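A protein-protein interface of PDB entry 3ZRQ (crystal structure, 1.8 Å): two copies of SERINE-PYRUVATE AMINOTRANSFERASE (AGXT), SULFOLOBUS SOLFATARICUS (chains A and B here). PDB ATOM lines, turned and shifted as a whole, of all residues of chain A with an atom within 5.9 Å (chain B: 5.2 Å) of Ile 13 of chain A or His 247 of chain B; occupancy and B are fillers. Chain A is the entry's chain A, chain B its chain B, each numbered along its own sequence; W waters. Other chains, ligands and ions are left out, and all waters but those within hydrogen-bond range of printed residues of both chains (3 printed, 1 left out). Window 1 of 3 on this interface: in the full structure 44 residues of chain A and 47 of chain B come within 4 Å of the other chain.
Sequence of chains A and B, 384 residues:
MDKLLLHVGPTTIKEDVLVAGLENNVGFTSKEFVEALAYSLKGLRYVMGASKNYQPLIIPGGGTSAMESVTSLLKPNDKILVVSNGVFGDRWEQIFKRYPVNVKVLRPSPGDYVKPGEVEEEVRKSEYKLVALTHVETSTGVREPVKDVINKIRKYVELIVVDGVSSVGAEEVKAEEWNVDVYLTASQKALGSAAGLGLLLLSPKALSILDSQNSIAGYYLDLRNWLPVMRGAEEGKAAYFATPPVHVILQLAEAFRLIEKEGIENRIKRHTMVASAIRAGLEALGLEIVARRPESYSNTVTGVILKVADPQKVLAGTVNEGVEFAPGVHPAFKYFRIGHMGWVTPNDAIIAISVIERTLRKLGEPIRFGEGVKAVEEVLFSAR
Position printed for both chains: 251.
Printed residues of chain B that touch a printed residue of chain A: Gly 21, Leu 22, Glu 23, Asn 24, Val 26, Pro 245 and His 247. Hydrophobic or aromatic side chains of chain B within 4 Å of the printed part of chain A: Leu 22, Pro 245 and His 247. Of the 14 printed residues of chain A, 6 touch a printed residue of chain B. Among the printed residues, no Asp or Glu carboxylate lies within 4 Å of a Lys or Arg side-chain nitrogen of the other chain.
The backbone NH (N) of Ile 13 of chain A sits at hydrogen-bond distance from the backbone carbonyl oxygen (O) of Asn 24 of chain B (2.9 Å).
Water W2 lies within hydrogen-bond range of a ring nitrogen (ND1) of His 247 of chain B (2.6 Å) and the backbone NH (N) of Ala 195 of chain A (2.8 Å). Water W3 lies within hydrogen-bond range of the side-chain amide nitrogen of Gln 251 of chain A (2.8 Å) and the backbone carbonyl oxygen of Gly 21 of chain B (2.9 Å). Water W1 lies within hydrogen-bond range of O of Ala 195 of chain A (2.8 Å), N of Val 248 of chain B (3.2 Å) and N of His 247 of chain B (3.2 Å).
Glu 15 of chain A touches none of the printed residues of chain B. Of the printed residues of chain B, Leu 18 of chain A touches Gly 21 (3.8 Å), Leu 22 (3.8 Å), Glu 23 (3.7 Å) and Asn 24 (3.8 Å). Of the printed residues of chain B, Ala 195 of chain A touches Pro 245. Printed residues of chain A within 4 Å of Gly 21 of chain B: Leu 18 (3.8 Å). Printed residues of chain A within 4 Å of Leu 22 of chain B: Leu 18. Of the printed residues of chain A, Val 26 of chain B touches Pro 10 (3.8 Å). His 247 of chain B touches just one residue of chain A: Ile 13 (3.7 Å). The nearest printed residue of chain B that does not touch Ile 13 of chain A is Asn 25 of chain B (5.2 Å). The nearest residue of chain A that does not touch His 247 of chain B is Leu 18 of chain A (4.2 Å). The nearest printed residue of chain B that does not touch Thr 12 of chain A is Asn 25 of chain B (5.0 Å).
The backbone carbonyl oxygen of Leu 18 of chain A sits at hydrogen-bond distance from the side-chain amide nitrogen of Gln 251 of chain A, 3.1 Å away. A ring nitrogen (NE2) of His 247 of chain B lies within hydrogen-bond range of the backbone carbonyl oxygen (O) of Glu 23 of chain B (2.7 Å).
Val 26 of chain B touches Pro 10 of chain A. Asn 24 of chain B touches Thr 11 of chain A (O to O, 3.8 Å). CA of Thr 12 of chain A touches O of Asn 24 of chain B, at 3.4 Å. His 247 of chain B touches Ile 13 of chain A (CE1 to CD1, 3.7 Å). Gly 21 of chain B touches Leu 18 of chain A (O to CD1, 3.8 Å). Leu 22 of chain B touches Leu 18 of chain A (CD2 to O, 3.8 Å). CD1 of Leu 18 of chain A touches O of Glu 23 of chain B, at 3.7 Å. Asn 24 of chain B touches Leu 18 of chain A. O of Ala 195 of chain A touches CA of Pro 245 of chain B, at 3.7 Å.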
ATOM      1  N   PRO A  10       3.592   0.207 -15.518  1.00  0.00           N
ATOM      2  CA  PRO A  10       3.469  -0.675 -16.681  1.00  0.00           C
ATOM      3  C   PRO A  10       3.645   0.063 -18.014  1.00  0.00           C
ATOM      4  O   PRO A  10       3.396   1.274 -18.125  1.00  0.00           O
ATOM      5  CB  PRO A  10       2.033  -1.225 -16.577  1.00  0.00           C
ATOM      6  CG  PRO A  10       1.684  -1.138 -15.137  1.00  0.00           C
ATOM      7  CD  PRO A  10       2.480   0.019 -14.559  1.00  0.00           C
ATOM      8  N   THR A  11       4.102  -0.689 -19.001  1.00  0.00           N
ATOM      9  CA  THR A  11       4.114  -0.262 -20.386  1.00  0.00           C
ATOM     10  C   THR A  11       3.076  -1.191 -21.042  1.00  0.00           C
ATOM     11  O   THR A  11       2.268  -1.795 -20.328  1.00  0.00           O
ATOM     12  CB  THR A  11       5.559  -0.390 -20.962  1.00  0.00           C
ATOM     13  OG1 THR A  11       5.535  -0.360 -22.395  1.00  0.00           O
ATOM     14  CG2 THR A  11       6.248  -1.692 -20.458  1.00  0.00           C
ATOM     15  N   THR A  12       3.063  -1.303 -22.367  1.00  0.00           N
ATOM     16  CA  THR A  12       2.132  -2.225 -23.025  1.00  0.00           C
ATOM     17  C   THR A  12       2.512  -3.664 -22.643  1.00  0.00           C
ATOM     18  O   THR A  12       3.685  -4.058 -22.764  1.00  0.00           O
ATOM     19  CB  THR A  12       2.120  -2.030 -24.562  1.00  0.00           C
ATOM     20  OG1 THR A  12       1.908  -0.647 -24.861  1.00  0.00           O
ATOM     21  CG2 THR A  12       0.986  -2.848 -25.204  1.00  0.00           C
ATOM     22  N   ILE A  13       1.542  -4.432 -22.144  1.00  0.00           N
ATOM     23  CA  ILE A  13       1.804  -5.818 -21.754  1.00  0.00           C
ATOM     24  C   ILE A  13       1.340  -6.789 -22.859  1.00  0.00           C
ATOM     25  O   ILE A  13       0.248  -6.672 -23.356  1.00  0.00           O
ATOM     26  CB  ILE A  13       1.127  -6.164 -20.405  1.00  0.00           C
ATOM     27  CG1 ILE A  13       1.552  -5.130 -19.324  1.00  0.00           C
ATOM     28  CG2 ILE A  13       1.490  -7.591 -20.005  1.00  0.00           C
ATOM     29  CD1 ILE A  13       0.905  -5.315 -17.983  1.00  0.00           C
ATOM     30  N   LYS A  14       2.188  -7.740 -23.252  1.00  0.00           N
ATOM     31  CA  LYS A  14       1.772  -8.794 -24.201  1.00  0.00           C
ATOM     32  C   LYS A  14       0.526  -9.535 -23.709  1.00  0.00           C
ATOM     33  O   LYS A  14       0.397  -9.822 -22.504  1.00  0.00           O
ATOM     34  CB  LYS A  14       2.901  -9.794 -24.433  1.00  0.00           C
ATOM     35  CG  LYS A  14       3.656  -9.647 -25.730  1.00  0.00           C
ATOM     36  CD  LYS A  14       4.435 -10.932 -26.003  1.00  0.00           C
ATOM     37  CE  LYS A  14       5.029 -10.960 -27.401  1.00  0.00           C
ATOM     38  NZ  LYS A  14       5.426 -12.360 -27.757  1.00  0.00           N
ATOM     39  N   GLU A  15      -0.390  -9.829 -24.639  1.00  0.00           N
ATOM     40  CA  GLU A  15      -1.660 -10.499 -24.324  1.00  0.00           C
ATOM     41  C   GLU A  15      -1.418 -11.841 -23.660  1.00  0.00           C
ATOM     42  O   GLU A  15      -2.121 -12.197 -22.717  1.00  0.00           O
ATOM     43  CB  GLU A  15      -2.531 -10.695 -25.588  1.00  0.00           C
ATOM     44  CG  GLU A  15      -3.965 -11.204 -25.325  1.00  0.00           C
ATOM     45  CD  GLU A  15      -4.690 -11.701 -26.586  1.00  0.00           C
ATOM     46  OE1 GLU A  15      -4.032 -11.906 -27.637  1.00  0.00           O
ATOM     47  OE2 GLU A  15      -5.927 -11.887 -26.523  1.00  0.00           O
ATOM     48  N   VAL A  17       0.907 -12.704 -21.776  1.00  0.00           N
ATOM     49  CA  VAL A  17       1.296 -12.480 -20.375  1.00  0.00           C
ATOM     50  C   VAL A  17       0.060 -12.281 -19.502  1.00  0.00           C
ATOM     51  O   VAL A  17      -0.116 -12.988 -18.517  1.00  0.00           O
ATOM     52  CB  VAL A  17       2.329 -11.335 -20.217  1.00  0.00           C
ATOM     53  CG1 VAL A  17       2.702 -11.120 -18.751  1.00  0.00           C
ATOM     54  CG2 VAL A  17       3.589 -11.675 -20.994  1.00  0.00           C
ATOM     55  N   LEU A  18      -0.810 -11.351 -19.880  1.00  0.00           N
ATOM     56  CA  LEU A  18      -2.024 -11.143 -19.094  1.00  0.00           C
ATOM     57  C   LEU A  18      -2.930 -12.370 -18.987  1.00  0.00           C
ATOM     58  O   LEU A  18      -3.476 -12.666 -17.914  1.00  0.00           O
ATOM     59  CB  LEU A  18      -2.791  -9.919 -19.576  1.00  0.00           C
ATOM     60  CG  LEU A  18      -2.141  -8.557 -19.282  1.00  0.00           C
ATOM     61  CD1 LEU A  18      -3.122  -7.467 -19.643  1.00  0.00           C
ATOM     62  CD2 LEU A  18      -1.662  -8.337 -17.829  1.00  0.00           C
ATOM     63  N   GLY A 192       8.214  -6.367 -18.509  1.00  0.00           N
ATOM     64  CA  GLY A 192       7.003  -6.295 -19.323  1.00  0.00           C
ATOM     65  C   GLY A 192       5.798  -7.028 -18.774  1.00  0.00           C
ATOM     66  O   GLY A 192       4.924  -7.396 -19.544  1.00  0.00           O
ATOM     67  N   SER A 193       5.740  -7.232 -17.459  1.00  0.00           N
ATOM     68  CA  SER A 193       4.623  -7.966 -16.839  1.00  0.00           C
ATOM     69  C   SER A 193       3.720  -7.061 -16.002  1.00  0.00           C
ATOM     70  O   SER A 193       3.854  -5.827 -16.017  1.00  0.00           O
ATOM     71  CB  SER A 193       5.139  -9.158 -16.011  1.00  0.00           C
ATOM     72  OG  SER A 193       4.074  -9.998 -15.654  1.00  0.00           O
ATOM     73  N   ALA A 194       2.753  -7.659 -15.313  1.00  0.00           N
ATOM     74  CA  ALA A 194       1.834  -6.882 -14.477  1.00  0.00           C
ATOM     75  C   ALA A 194       2.560  -6.409 -13.208  1.00  0.00           C
ATOM     76  O   ALA A 194       3.455  -7.099 -12.704  1.00  0.00           O
ATOM     77  CB  ALA A 194       0.616  -7.729 -14.094  1.00  0.00           C
ATOM     78  N   ALA A 195       2.165  -5.238 -12.719  1.00  0.00           N
ATOM     79  CA  ALA A 195       2.705  -4.658 -11.475  1.00  0.00           C
ATOM     80  C   ALA A 195       2.249  -5.441 -10.225  1.00  0.00           C
ATOM     81  O   ALA A 195       1.196  -6.113 -10.241  1.00  0.00           O
ATOM     82  CB  ALA A 195       2.262  -3.197 -11.356  1.00  0.00           C
ATOM     83  N   GLN A 251       1.491 -14.503 -14.214  1.00  0.00           N
ATOM     84  CA  GLN A 251       1.819 -13.641 -15.346  1.00  0.00           C
ATOM     85  C   GLN A 251       3.333 -13.459 -15.478  1.00  0.00           C
ATOM     86  O   GLN A 251       3.871 -13.569 -16.584  1.00  0.00           O
ATOM     87  CB  GLN A 251       1.071 -12.317 -15.230  1.00  0.00           C
ATOM     88  CG  GLN A 251      -0.449 -12.532 -15.250  1.00  0.00           C
ATOM     89  CD  GLN A 251      -1.267 -11.313 -14.844  1.00  0.00           C
ATOM     90  OE1 GLN A 251      -1.019 -10.691 -13.815  1.00  0.00           O
ATOM     91  NE2 GLN A 251      -2.285 -11.001 -15.631  1.00  0.00           N
ATOM     92  N   TRP A 343       8.294  -5.062 -24.312  1.00  0.00           N
ATOM     93  CA  TRP A 343       7.926  -5.710 -25.593  1.00  0.00           C
ATOM     94  C   TRP A 343       8.036  -4.738 -26.767  1.00  0.00           C
ATOM     95  O   TRP A 343       7.540  -5.026 -27.852  1.00  0.00           O
ATOM     96  CB  TRP A 343       6.495  -6.288 -25.510  1.00  0.00           C
ATOM     97  CG  TRP A 343       6.264  -7.068 -24.255  1.00  0.00           C
ATOM     98  CD1 TRP A 343       5.425  -6.732 -23.222  1.00  0.00           C
ATOM     99  CD2 TRP A 343       6.894  -8.300 -23.879  1.00  0.00           C
ATOM    100  NE1 TRP A 343       5.493  -7.685 -22.228  1.00  0.00           N
ATOM    101  CE2 TRP A 343       6.394  -8.651 -22.597  1.00  0.00           C
ATOM    102  CE3 TRP A 343       7.845  -9.137 -24.489  1.00  0.00           C
ATOM    103  CZ2 TRP A 343       6.815  -9.798 -21.911  1.00  0.00           C
ATOM    104  CZ3 TRP A 343       8.244 -10.290 -23.823  1.00  0.00           C
ATOM    105  CH2 TRP A 343       7.730 -10.617 -22.548  1.00  0.00           C
ATOM    106  N   GLY B  21      -9.066  -7.863 -15.366  1.00  0.00           N
ATOM    107  CA  GLY B  21      -7.633  -7.579 -15.375  1.00  0.00           C
ATOM    108  C   GLY B  21      -6.948  -7.680 -16.730  1.00  0.00           C
ATOM    109  O   GLY B  21      -5.724  -7.594 -16.817  1.00  0.00           O
ATOM    110  N   LEU B  22      -7.727  -7.875 -17.792  1.00  0.00           N
ATOM    111  CA  LEU B  22      -7.170  -8.029 -19.133  1.00  0.00           C
ATOM    112  C   LEU B  22      -7.215  -6.740 -19.925  1.00  0.00           C
ATOM    113  O   LEU B  22      -7.951  -6.644 -20.909  1.00  0.00           O
ATOM    114  CB  LEU B  22      -7.952  -9.108 -19.908  1.00  0.00           C
ATOM    115  CG  LEU B  22      -7.927 -10.541 -19.394  1.00  0.00           C
ATOM    116  CD1 LEU B  22      -8.920 -11.390 -20.192  1.00  0.00           C
ATOM    117  CD2 LEU B  22      -6.520 -11.100 -19.543  1.00  0.00           C
ATOM    118  N   GLU B  23      -6.466  -5.740 -19.497  1.00  0.00           N
ATOM    119  CA  GLU B  23      -6.390  -4.459 -20.209  1.00  0.00           C
ATOM    120  C   GLU B  23      -4.912  -4.188 -20.384  1.00  0.00           C
ATOM    121  O   GLU B  23      -4.237  -3.915 -19.402  1.00  0.00           O
ATOM    122  CB  GLU B  23      -6.991  -3.348 -19.365  1.00  0.00           C
ATOM    123  CG  GLU B  23      -8.375  -3.612 -18.856  1.00  0.00           C
ATOM    124  CD  GLU B  23      -9.439  -3.098 -19.798  1.00  0.00           C
ATOM    125  OE1 GLU B  23      -9.087  -2.641 -20.910  1.00  0.00           O
ATOM    126  OE2 GLU B  23     -10.627  -3.160 -19.422  1.00  0.00           O
ATOM    127  N   ASN B  24      -4.392  -4.290 -21.605  1.00  0.00           N
ATOM    128  CA  ASN B  24      -2.932  -4.356 -21.770  1.00  0.00           C
ATOM    129  C   ASN B  24      -2.187  -3.004 -21.832  1.00  0.00           C
ATOM    130  O   ASN B  24      -0.962  -2.974 -21.933  1.00  0.00           O
ATOM    131  CB  ASN B  24      -2.575  -5.250 -22.953  1.00  0.00           C
ATOM    132  CG  ASN B  24      -2.837  -4.589 -24.285  1.00  0.00           C
ATOM    133  OD1 ASN B  24      -3.739  -3.751 -24.425  1.00  0.00           O
ATOM    134  ND2 ASN B  24      -2.030  -4.946 -25.275  1.00  0.00           N
ATOM    135  N   ASN B  25      -2.941  -1.910 -21.738  1.00  0.00           N
ATOM    136  CA  ASN B  25      -2.416  -0.557 -21.907  1.00  0.00           C
ATOM    137  C   ASN B  25      -2.875   0.402 -20.806  1.00  0.00           C
ATOM    138  O   ASN B  25      -3.149   1.567 -21.068  1.00  0.00           O
ATOM    139  CB  ASN B  25      -2.838  -0.015 -23.283  1.00  0.00           C
ATOM    140  CG  ASN B  25      -4.350   0.040 -23.445  1.00  0.00           C
ATOM    141  OD1 ASN B  25      -5.094  -0.516 -22.626  1.00  0.00           O
ATOM    142  ND2 ASN B  25      -4.816   0.731 -24.490  1.00  0.00           N
ATOM    143  N   VAL B  26      -2.961  -0.095 -19.579  1.00  0.00           N
ATOM    144  CA  VAL B  26      -3.392   0.682 -18.413  1.00  0.00           C
ATOM    145  C   VAL B  26      -2.219   0.766 -17.417  1.00  0.00           C
ATOM    146  O   VAL B  26      -1.547  -0.233 -17.153  1.00  0.00           O
ATOM    147  CB  VAL B  26      -4.634   0.017 -17.753  1.00  0.00           C
ATOM    148  CG1 VAL B  26      -5.016   0.704 -16.444  1.00  0.00           C
ATOM    149  CG2 VAL B  26      -5.820   0.018 -18.729  1.00  0.00           C
ATOM    150  N   PRO B 245      -0.520  -2.457  -7.501  1.00  0.00           N
ATOM    151  CA  PRO B 245      -0.806  -3.581  -8.384  1.00  0.00           C
ATOM    152  C   PRO B 245      -2.019  -3.189  -9.285  1.00  0.00           C
ATOM    153  O   PRO B 245      -3.152  -3.533  -8.978  1.00  0.00           O
ATOM    154  CB  PRO B 245      -1.212  -4.706  -7.409  1.00  0.00           C
ATOM    155  CG  PRO B 245      -0.654  -4.276  -6.036  1.00  0.00           C
ATOM    156  CD  PRO B 245      -0.840  -2.772  -6.090  1.00  0.00           C
ATOM    157  N   VAL B 246      -1.736  -2.428 -10.343  1.00  0.00           N
ATOM    158  CA  VAL B 246      -2.755  -1.772 -11.185  1.00  0.00           C
ATOM    159  C   VAL B 246      -3.883  -2.725 -11.616  1.00  0.00           C
ATOM    160  O   VAL B 246      -5.057  -2.431 -11.412  1.00  0.00           O
ATOM    161  CB  VAL B 246      -2.091  -1.110 -12.423  1.00  0.00           C
ATOM    162  CG1 VAL B 246      -3.127  -0.705 -13.466  1.00  0.00           C
ATOM    163  CG2 VAL B 246      -1.275   0.079 -11.997  1.00  0.00           C
ATOM    164  N   HIS B 247      -3.505  -3.852 -12.205  1.00  0.00           N
ATOM    165  CA  HIS B 247      -4.463  -4.824 -12.735  1.00  0.00           C
ATOM    166  C   HIS B 247      -5.209  -5.571 -11.629  1.00  0.00           C
ATOM    167  O   HIS B 247      -6.390  -5.876 -11.775  1.00  0.00           O
ATOM    168  CB  HIS B 247      -3.787  -5.765 -13.737  1.00  0.00           C
ATOM    169  CG  HIS B 247      -3.346  -5.072 -14.992  1.00  0.00           C
ATOM    170  ND1 HIS B 247      -2.163  -4.371 -15.075  1.00  0.00           N
ATOM    171  CD2 HIS B 247      -3.930  -4.972 -16.212  1.00  0.00           C
ATOM    172  CE1 HIS B 247      -2.039  -3.861 -16.291  1.00  0.00           C
ATOM    173  NE2 HIS B 247      -3.096  -4.218 -17.002  1.00  0.00           N
ATOM    174  N   VAL B 248      -4.560  -5.793 -10.486  1.00  0.00           N
ATOM    175  CA  VAL B 248      -5.276  -6.395  -9.326  1.00  0.00           C
ATOM    176  C   VAL B 248      -6.370  -5.440  -8.852  1.00  0.00           C
ATOM    177  O   VAL B 248      -7.392  -5.876  -8.350  1.00  0.00           O
ATOM    178  CB  VAL B 248      -4.315  -6.679  -8.150  1.00  0.00           C
ATOM    179  CG1 VAL B 248      -5.053  -7.256  -6.940  1.00  0.00           C
ATOM    180  CG2 VAL B 248      -3.282  -7.726  -8.624  1.00  0.00           C
ATOM    181  N   ILE B 249      -6.089  -4.151  -8.957  1.00  0.00           N
ATOM    182  CA  ILE B 249      -7.072  -3.131  -8.563  1.00  0.00           C
ATOM    183  C   ILE B 249      -8.262  -3.069  -9.572  1.00  0.00           C
ATOM    184  O   ILE B 249      -9.434  -2.858  -9.169  1.00  0.00           O
ATOM    185  CB  ILE B 249      -6.415  -1.756  -8.345  1.00  0.00           C
ATOM    186  CG1 ILE B 249      -5.528  -1.786  -7.072  1.00  0.00           C
ATOM    187  CG2 ILE B 249      -7.511  -0.640  -8.206  1.00  0.00           C
ATOM    188  CD1 ILE B 249      -4.607  -0.607  -6.861  1.00  0.00           C
ATOM    189  N   LEU B 250      -7.960  -3.244 -10.854  1.00  0.00           N
ATOM    190  CA  LEU B 250      -9.040  -3.387 -11.875  1.00  0.00           C
ATOM    191  C   LEU B 250      -9.976  -4.546 -11.497  1.00  0.00           C
ATOM    192  O   LEU B 250     -11.208  -4.415 -11.537  1.00  0.00           O
ATOM    193  CB  LEU B 250      -8.451  -3.583 -13.283  1.00  0.00           C
ATOM    194  CG  LEU B 250      -7.639  -2.445 -13.896  1.00  0.00           C
ATOM    195  CD1 LEU B 250      -7.097  -2.794 -15.291  1.00  0.00           C
ATOM    196  CD2 LEU B 250      -8.489  -1.177 -13.972  1.00  0.00           C
ATOM    197  N   GLN B 251      -9.385  -5.684 -11.130  1.00  0.00           N
ATOM    198  CA  GLN B 251     -10.155  -6.844 -10.711  1.00  0.00           C
ATOM    199  C   GLN B 251     -10.965  -6.555  -9.447  1.00  0.00           C
ATOM    200  O   GLN B 251     -12.158  -6.884  -9.389  1.00  0.00           O
ATOM    201  CB  GLN B 251      -9.238  -8.066 -10.561  1.00  0.00           C
ATOM    202  CG  GLN B 251      -8.555  -8.413 -11.877  1.00  0.00           C
ATOM    203  CD  GLN B 251      -7.421  -9.448 -11.742  1.00  0.00           C
ATOM    204  OE1 GLN B 251      -6.512  -9.286 -10.930  1.00  0.00           O
ATOM    205  NE2 GLN B 251      -7.440 -10.462 -12.598  1.00  0.00           N
ATOM    206  N   LEU B 252     -10.338  -5.934  -8.438  1.00  0.00           N
ATOM    207  CA  LEU B 252     -11.065  -5.579  -7.219  1.00  0.00           C
ATOM    208  C   LEU B 252     -12.318  -4.719  -7.513  1.00  0.00           C
ATOM    209  O   LEU B 252     -13.368  -4.937  -6.887  1.00  0.00           O
ATOM    210  CB  LEU B 252     -10.144  -4.833  -6.207  1.00  0.00           C
ATOM    211  CG  LEU B 252     -10.761  -4.403  -4.852  1.00  0.00           C
ATOM    212  CD1 LEU B 252     -11.246  -5.624  -4.021  1.00  0.00           C
ATOM    213  CD2 LEU B 252      -9.798  -3.563  -4.056  1.00  0.00           C
HETATM  214  O   HOH W   1      -1.469  -6.131 -11.197  1.00  0.00           O
HETATM  215  O   HOH W   2      -0.254  -4.018 -13.352  1.00  0.00           O
HETATM  216  O   HOH W   3      -4.157  -9.089 -14.952  1.00  0.00           O
